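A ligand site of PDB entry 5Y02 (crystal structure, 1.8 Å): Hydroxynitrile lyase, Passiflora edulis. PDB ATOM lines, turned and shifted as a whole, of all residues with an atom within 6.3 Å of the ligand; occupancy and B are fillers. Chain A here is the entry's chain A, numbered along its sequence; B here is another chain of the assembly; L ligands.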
ATOM      1  N   HIS A   9      32.254   9.482  14.783  1.00  0.00           N
ATOM      2  CA  HIS A   9      31.915  10.125  16.046  1.00  0.00           C
ATOM      3  C   HIS A   9      30.468   9.726  16.332  1.00  0.00           C
ATOM      4  O   HIS A   9      29.542  10.163  15.637  1.00  0.00           O
ATOM      5  CB  HIS A   9      32.077  11.644  15.883  1.00  0.00           C
ATOM      6  CG  HIS A   9      31.620  12.460  17.046  1.00  0.00           C
ATOM      7  ND1 HIS A   9      32.320  12.520  18.234  1.00  0.00           N
ATOM      8  CD2 HIS A   9      30.595  13.335  17.169  1.00  0.00           C
ATOM      9  CE1 HIS A   9      31.712  13.364  19.060  1.00  0.00           C
ATOM     10  NE2 HIS A   9      30.669  13.867  18.441  1.00  0.00           N
ATOM     11  N   VAL A  11      27.457   9.273  19.258  1.00  0.00           N
ATOM     12  CA  VAL A  11      26.921   9.771  20.510  1.00  0.00           C
ATOM     13  C   VAL A  11      25.627   9.020  20.790  1.00  0.00           C
ATOM     14  O   VAL A  11      24.747   8.924  19.919  1.00  0.00           O
ATOM     15  CB  VAL A  11      26.616  11.272  20.408  1.00  0.00           C
ATOM     16  CG1 VAL A  11      26.007  11.813  21.702  1.00  0.00           C
ATOM     17  CG2 VAL A  11      27.889  12.030  20.036  1.00  0.00           C
ATOM     18  N   TYR A  31      21.959  20.730  16.563  1.00  0.00           N
ATOM     19  CA  TYR A  31      23.061  19.797  16.370  1.00  0.00           C
ATOM     20  C   TYR A  31      23.288  19.554  14.868  1.00  0.00           C
ATOM     21  O   TYR A  31      24.403  19.727  14.385  1.00  0.00           O
ATOM     22  CB  TYR A  31      22.734  18.472  17.059  1.00  0.00           C
ATOM     23  CG  TYR A  31      23.853  17.480  17.260  1.00  0.00           C
ATOM     24  CD1 TYR A  31      25.135  17.654  16.734  1.00  0.00           C
ATOM     25  CD2 TYR A  31      23.591  16.315  17.961  1.00  0.00           C
ATOM     26  CE1 TYR A  31      26.120  16.699  16.914  1.00  0.00           C
ATOM     27  CE2 TYR A  31      24.572  15.360  18.155  1.00  0.00           C
ATOM     28  CZ  TYR A  31      25.816  15.549  17.627  1.00  0.00           C
ATOM     29  OH  TYR A  31      26.792  14.588  17.841  1.00  0.00           O
ATOM     30  N   LEU A  34      25.008  22.300  12.760  1.00  0.00           N
ATOM     31  CA  LEU A  34      26.459  22.449  12.833  1.00  0.00           C
ATOM     32  C   LEU A  34      27.177  22.044  11.560  1.00  0.00           C
ATOM     33  O   LEU A  34      28.221  22.609  11.280  1.00  0.00           O
ATOM     34  CB  LEU A  34      27.073  21.689  14.016  1.00  0.00           C
ATOM     35  CG  LEU A  34      26.848  22.267  15.412  1.00  0.00           C
ATOM     36  CD1 LEU A  34      27.402  21.313  16.477  1.00  0.00           C
ATOM     37  CD2 LEU A  34      27.473  23.634  15.566  1.00  0.00           C
ATOM     38  N   MET A  41      32.282  18.537  10.100  1.00  0.00           N
ATOM     39  CA  MET A  41      31.307  17.492  10.445  1.00  0.00           C
ATOM     40  C   MET A  41      30.540  17.042   9.220  1.00  0.00           C
ATOM     41  O   MET A  41      29.794  17.842   8.645  1.00  0.00           O
ATOM     42  CB  MET A  41      30.336  17.950  11.541  1.00  0.00           C
ATOM     43  CG  MET A  41      29.411  16.811  11.992  1.00  0.00           C
ATOM     44  SD  MET A  41      28.481  17.104  13.504  1.00  0.00           S
ATOM     45  CE  MET A  41      27.099  18.007  12.829  1.00  0.00           C
ATOM     46  N   TYR A  65      23.361   9.568  17.534  1.00  0.00           N
ATOM     47  CA  TYR A  65      23.795  10.554  16.533  1.00  0.00           C
ATOM     48  C   TYR A  65      25.149  10.091  15.988  1.00  0.00           C
ATOM     49  O   TYR A  65      26.062   9.763  16.758  1.00  0.00           O
ATOM     50  CB  TYR A  65      23.950  11.949  17.151  1.00  0.00           C
ATOM     51  CG  TYR A  65      22.867  12.312  18.131  1.00  0.00           C
ATOM     52  CD1 TYR A  65      22.922  11.849  19.443  1.00  0.00           C
ATOM     53  CD2 TYR A  65      21.783  13.106  17.759  1.00  0.00           C
ATOM     54  CE1 TYR A  65      21.956  12.159  20.362  1.00  0.00           C
ATOM     55  CE2 TYR A  65      20.795  13.428  18.694  1.00  0.00           C
ATOM     56  CZ  TYR A  65      20.891  12.956  20.001  1.00  0.00           C
ATOM     57  OH  TYR A  65      19.954  13.238  20.948  1.00  0.00           O
ATOM     58  N   SER A  67      28.302  10.912  13.021  1.00  0.00           N
ATOM     59  CA  SER A  67      28.924  11.821  12.040  1.00  0.00           C
ATOM     60  C   SER A  67      30.345  11.365  11.726  1.00  0.00           C
ATOM     61  O   SER A  67      30.914  10.471  12.395  1.00  0.00           O
ATOM     62  CB  SER A  67      28.886  13.261  12.530  1.00  0.00           C
ATOM     63  OG  SER A  67      29.428  13.411  13.813  1.00  0.00           O
ATOM     64  N   PHE A  75      38.410  16.951  13.554  1.00  0.00           N
ATOM     65  CA  PHE A  75      37.486  16.811  14.691  1.00  0.00           C
ATOM     66  C   PHE A  75      37.781  17.814  15.807  1.00  0.00           C
ATOM     67  O   PHE A  75      36.872  18.487  16.298  1.00  0.00           O
ATOM     68  CB  PHE A  75      37.485  15.384  15.269  1.00  0.00           C
ATOM     69  CG  PHE A  75      36.612  15.260  16.475  1.00  0.00           C
ATOM     70  CD1 PHE A  75      35.236  15.299  16.342  1.00  0.00           C
ATOM     71  CD2 PHE A  75      37.159  15.228  17.740  1.00  0.00           C
ATOM     72  CE1 PHE A  75      34.406  15.221  17.447  1.00  0.00           C
ATOM     73  CE2 PHE A  75      36.338  15.161  18.862  1.00  0.00           C
ATOM     74  CZ  PHE A  75      34.960  15.173  18.714  1.00  0.00           C
ATOM     75  N   PHE A  78      36.961  21.355  14.848  1.00  0.00           N
ATOM     76  CA  PHE A  78      35.504  21.433  14.987  1.00  0.00           C
ATOM     77  C   PHE A  78      35.046  21.582  16.442  1.00  0.00           C
ATOM     78  O   PHE A  78      34.321  22.523  16.794  1.00  0.00           O
ATOM     79  CB  PHE A  78      34.850  20.202  14.376  1.00  0.00           C
ATOM     80  CG  PHE A  78      33.397  20.033  14.729  1.00  0.00           C
ATOM     81  CD1 PHE A  78      32.417  20.771  14.062  1.00  0.00           C
ATOM     82  CD2 PHE A  78      33.004  19.133  15.730  1.00  0.00           C
ATOM     83  CE1 PHE A  78      31.068  20.610  14.379  1.00  0.00           C
ATOM     84  CE2 PHE A  78      31.664  18.977  16.056  1.00  0.00           C
ATOM     85  CZ  PHE A  78      30.696  19.719  15.384  1.00  0.00           C
ATOM     86  N   PHE A  79      35.495  20.657  17.296  1.00  0.00           N
ATOM     87  CA  PHE A  79      34.954  20.530  18.658  1.00  0.00           C
ATOM     88  C   PHE A  79      35.224  21.748  19.534  1.00  0.00           C
ATOM     89  O   PHE A  79      34.431  22.065  20.431  1.00  0.00           O
ATOM     90  CB  PHE A  79      35.481  19.247  19.317  1.00  0.00           C
ATOM     91  CG  PHE A  79      34.666  18.786  20.489  1.00  0.00           C
ATOM     92  CD1 PHE A  79      33.386  18.307  20.305  1.00  0.00           C
ATOM     93  CD2 PHE A  79      35.197  18.844  21.779  1.00  0.00           C
ATOM     94  CE1 PHE A  79      32.620  17.889  21.393  1.00  0.00           C
ATOM     95  CE2 PHE A  79      34.441  18.417  22.862  1.00  0.00           C
ATOM     96  CZ  PHE A  79      33.160  17.938  22.678  1.00  0.00           C
ATOM     97  N   PRO A  83      31.030  27.795  17.084  1.00  0.00           N
ATOM     98  CA  PRO A  83      29.689  27.195  17.005  1.00  0.00           C
ATOM     99  C   PRO A  83      29.507  25.921  17.854  1.00  0.00           C
ATOM    100  O   PRO A  83      28.455  25.738  18.473  1.00  0.00           O
ATOM    101  CB  PRO A  83      29.520  26.878  15.522  1.00  0.00           C
ATOM    102  CG  PRO A  83      30.462  27.803  14.817  1.00  0.00           C
ATOM    103  CD  PRO A  83      31.627  27.960  15.741  1.00  0.00           C
ATOM    104  N   ALA A  84      30.529  25.064  17.867  1.00  0.00           N
ATOM    105  CA  ALA A  84      30.494  23.840  18.667  1.00  0.00           C
ATOM    106  C   ALA A  84      30.480  24.168  20.141  1.00  0.00           C
ATOM    107  O   ALA A  84      29.749  23.536  20.892  1.00  0.00           O
ATOM    108  CB  ALA A  84      31.662  22.940  18.343  1.00  0.00           C
ATOM    109  N   LEU A  85      31.255  25.161  20.578  1.00  0.00           N
ATOM    110  CA  LEU A  85      31.258  25.509  21.990  1.00  0.00           C
ATOM    111  C   LEU A  85      29.910  26.082  22.426  1.00  0.00           C
ATOM    112  O   LEU A  85      29.465  25.826  23.550  1.00  0.00           O
ATOM    113  CB  LEU A  85      32.376  26.495  22.334  1.00  0.00           C
ATOM    114  CG  LEU A  85      33.814  25.995  22.190  1.00  0.00           C
ATOM    115  CD1 LEU A  85      34.741  27.189  22.317  1.00  0.00           C
ATOM    116  CD2 LEU A  85      34.163  24.927  23.214  1.00  0.00           C
ATOM    117  N   PHE A  87      26.977  25.315  21.015  1.00  0.00           N
ATOM    118  CA  PHE A  87      26.074  24.169  21.066  1.00  0.00           C
ATOM    119  C   PHE A  87      26.304  23.329  22.342  1.00  0.00           C
ATOM    120  O   PHE A  87      25.341  22.874  22.948  1.00  0.00           O
ATOM    121  CB  PHE A  87      26.217  23.314  19.816  1.00  0.00           C
ATOM    122  CG  PHE A  87      25.339  22.099  19.823  1.00  0.00           C
ATOM    123  CD1 PHE A  87      23.960  22.245  19.767  1.00  0.00           C
ATOM    124  CD2 PHE A  87      25.878  20.836  19.957  1.00  0.00           C
ATOM    125  CE1 PHE A  87      23.136  21.146  19.841  1.00  0.00           C
ATOM    126  CE2 PHE A  87      25.054  19.716  20.009  1.00  0.00           C
ATOM    127  CZ  PHE A  87      23.678  19.869  19.947  1.00  0.00           C
ATOM    128  N   ALA A  88      27.560  23.176  22.769  1.00  0.00           N
ATOM    129  CA  ALA A  88      27.887  22.375  23.979  1.00  0.00           C
ATOM    130  C   ALA A  88      27.192  22.907  25.226  1.00  0.00           C
ATOM    131  O   ALA A  88      26.830  22.127  26.108  1.00  0.00           O
ATOM    132  CB  ALA A  88      29.391  22.342  24.204  1.00  0.00           C
ATOM    133  N   PHE A  91      23.723  21.445  24.768  1.00  0.00           N
ATOM    134  CA  PHE A  91      23.615  20.004  24.616  1.00  0.00           C
ATOM    135  C   PHE A  91      23.971  19.203  25.882  1.00  0.00           C
ATOM    136  O   PHE A  91      23.174  18.384  26.312  1.00  0.00           O
ATOM    137  CB  PHE A  91      24.462  19.524  23.444  1.00  0.00           C
ATOM    138  CG  PHE A  91      24.297  18.071  23.150  1.00  0.00           C
ATOM    139  CD1 PHE A  91      23.088  17.585  22.677  1.00  0.00           C
ATOM    140  CD2 PHE A  91      25.342  17.181  23.363  1.00  0.00           C
ATOM    141  CE1 PHE A  91      22.910  16.235  22.408  1.00  0.00           C
ATOM    142  CE2 PHE A  91      25.183  15.827  23.098  1.00  0.00           C
ATOM    143  CZ  PHE A  91      23.979  15.362  22.619  1.00  0.00           C
ATOM    144  N   PHE A  92      25.154  19.424  26.447  1.00  0.00           N
ATOM    145  CA  PHE A  92      25.597  18.600  27.580  1.00  0.00           C
ATOM    146  C   PHE A  92      24.711  18.739  28.822  1.00  0.00           C
ATOM    147  O   PHE A  92      24.366  17.731  29.437  1.00  0.00           O
ATOM    148  CB  PHE A  92      27.098  18.825  27.887  1.00  0.00           C
ATOM    149  CG  PHE A  92      28.006  18.359  26.785  1.00  0.00           C
ATOM    150  CD1 PHE A  92      27.967  17.042  26.342  1.00  0.00           C
ATOM    151  CD2 PHE A  92      28.913  19.224  26.183  1.00  0.00           C
ATOM    152  CE1 PHE A  92      28.774  16.603  25.298  1.00  0.00           C
ATOM    153  CE2 PHE A  92      29.749  18.792  25.159  1.00  0.00           C
ATOM    154  CZ  PHE A  92      29.678  17.475  24.717  1.00  0.00           C
ATOM    155  N   ILE A  98      25.069  10.321  28.762  1.00  0.00           N
ATOM    156  CA  ILE A  98      25.684  10.395  27.438  1.00  0.00           C
ATOM    157  C   ILE A  98      26.861   9.427  27.392  1.00  0.00           C
ATOM    158  O   ILE A  98      27.540   9.215  28.399  1.00  0.00           O
ATOM    159  CB  ILE A  98      26.116  11.831  27.102  1.00  0.00           C
ATOM    160  CG1 ILE A  98      26.627  11.931  25.655  1.00  0.00           C
ATOM    161  CG2 ILE A  98      27.170  12.343  28.083  1.00  0.00           C
ATOM    162  CD1 ILE A  98      26.948  13.329  25.216  1.00  0.00           C
ATOM    163  N   VAL A 100      29.998   8.692  24.315  1.00  0.00           N
ATOM    164  CA  VAL A 100      30.545   9.091  23.008  1.00  0.00           C
ATOM    165  C   VAL A 100      31.773   8.250  22.710  1.00  0.00           C
ATOM    166  O   VAL A 100      32.664   8.157  23.529  1.00  0.00           O
ATOM    167  CB  VAL A 100      30.931  10.586  22.994  1.00  0.00           C
ATOM    168  CG1 VAL A 100      31.299  11.026  21.590  1.00  0.00           C
ATOM    169  CG2 VAL A 100      29.776  11.455  23.517  1.00  0.00           C
ATOM    170  N   GLU B  55      38.462  12.790  23.143  1.00  0.00           N
ATOM    171  CA  GLU B  55      37.287  13.128  23.937  1.00  0.00           C
ATOM    172  C   GLU B  55      37.157  12.109  25.053  1.00  0.00           C
ATOM    173  O   GLU B  55      37.490  10.952  24.846  1.00  0.00           O
ATOM    174  CB  GLU B  55      36.029  13.113  23.057  1.00  0.00           C
ATOM    175  CG  GLU B  55      34.766  13.573  23.758  1.00  0.00           C
ATOM    176  CD  GLU B  55      33.583  13.812  22.839  1.00  0.00           C
ATOM    177  OE1 GLU B  55      33.646  13.487  21.629  1.00  0.00           O
ATOM    178  OE2 GLU B  55      32.550  14.322  23.350  1.00  0.00           O
ATOM    179  N   ARG B  57      34.436  10.791  27.007  1.00  0.00           N
ATOM    180  CA  ARG B  57      33.038  10.489  27.308  1.00  0.00           C
ATOM    181  C   ARG B  57      32.669   9.068  26.927  1.00  0.00           C
ATOM    182  O   ARG B  57      31.495   8.752  26.807  1.00  0.00           O
ATOM    183  CB  ARG B  57      32.125  11.502  26.608  1.00  0.00           C
ATOM    184  CG  ARG B  57      32.261  12.917  27.193  1.00  0.00           C
ATOM    185  CD  ARG B  57      31.237  13.843  26.578  1.00  0.00           C
ATOM    186  NE  ARG B  57      31.329  15.235  27.046  1.00  0.00           N
ATOM    187  CZ  ARG B  57      30.692  15.752  28.110  1.00  0.00           C
ATOM    188  NH1 ARG B  57      29.903  15.030  28.894  1.00  0.00           N
ATOM    189  NH2 ARG B  57      30.858  17.054  28.385  1.00  0.00           N
HETATM  190  C1  LIG L   1      28.866  17.516  20.214  1.00  0.00           C
HETATM  191  C2  LIG L   1      28.691  18.147  21.433  1.00  0.00           C
HETATM  192  C3  LIG L   1      29.029  19.495  21.591  1.00  0.00           C
HETATM  193  C4  LIG L   1      29.515  20.211  20.505  1.00  0.00           C
HETATM  194  C5  LIG L   1      29.703  19.585  19.282  1.00  0.00           C
HETATM  195  C6  LIG L   1      29.378  18.242  19.119  1.00  0.00           C
HETATM  196  C7  LIG L   1      28.537  16.070  20.110  1.00  0.00           C
HETATM  197  C8  LIG L   1      29.437  15.385  21.063  1.00  0.00           C
HETATM  198  N1  LIG L   1      30.163  14.860  21.817  1.00  0.00           N
HETATM  199  O1  LIG L   1      28.768  15.583  18.778  1.00  0.00           O
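O1 of the ligand is in hydrogen-bond range of OH of Tyr 31 (2.4 Å). A ring nitrogen (NE2) of His 9 is in hydrogen-bond range of an oxygen (O1) of the ligand, 2.6 Å away. The side-chain carboxylate of Glu 55 of chain B is in hydrogen-bond range of a nitrogen (N1) of the ligand.
The backbone NH (N) of His 9 lies within hydrogen-bond range of the backbone carbonyl oxygen (O) of Ser 67 (2.9 Å). The side-chain carboxylate of Glu 55 of chain B lies within salt-bridge range of the guanidinium group of Arg 57 of chain B. The backbone carbonyl oxygen (O) of Arg 57 of chain B sits at hydrogen-bond distance from the backbone NH (N) of Val 100 (2.9 Å). O of Val 11 lies within hydrogen-bond range of N of Tyr 65 (2.8 Å).
Merely in contact with the ligand: Ala 84, Phe 92, Phe 87, Phe 78, Val 100, Val 11, Ala 88, Phe 79 and Phe 91. Hydrophobic or aromatic side chains that line the ligand: His 9, Val 11, Tyr 31, Phe 78, Phe 79, Ala 84, Phe 87, Ala 88, Phe 91, Phe 92 and Val 100. The nearest printed residue that does not touch the ligand is Leu 34 (4.02 Å).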
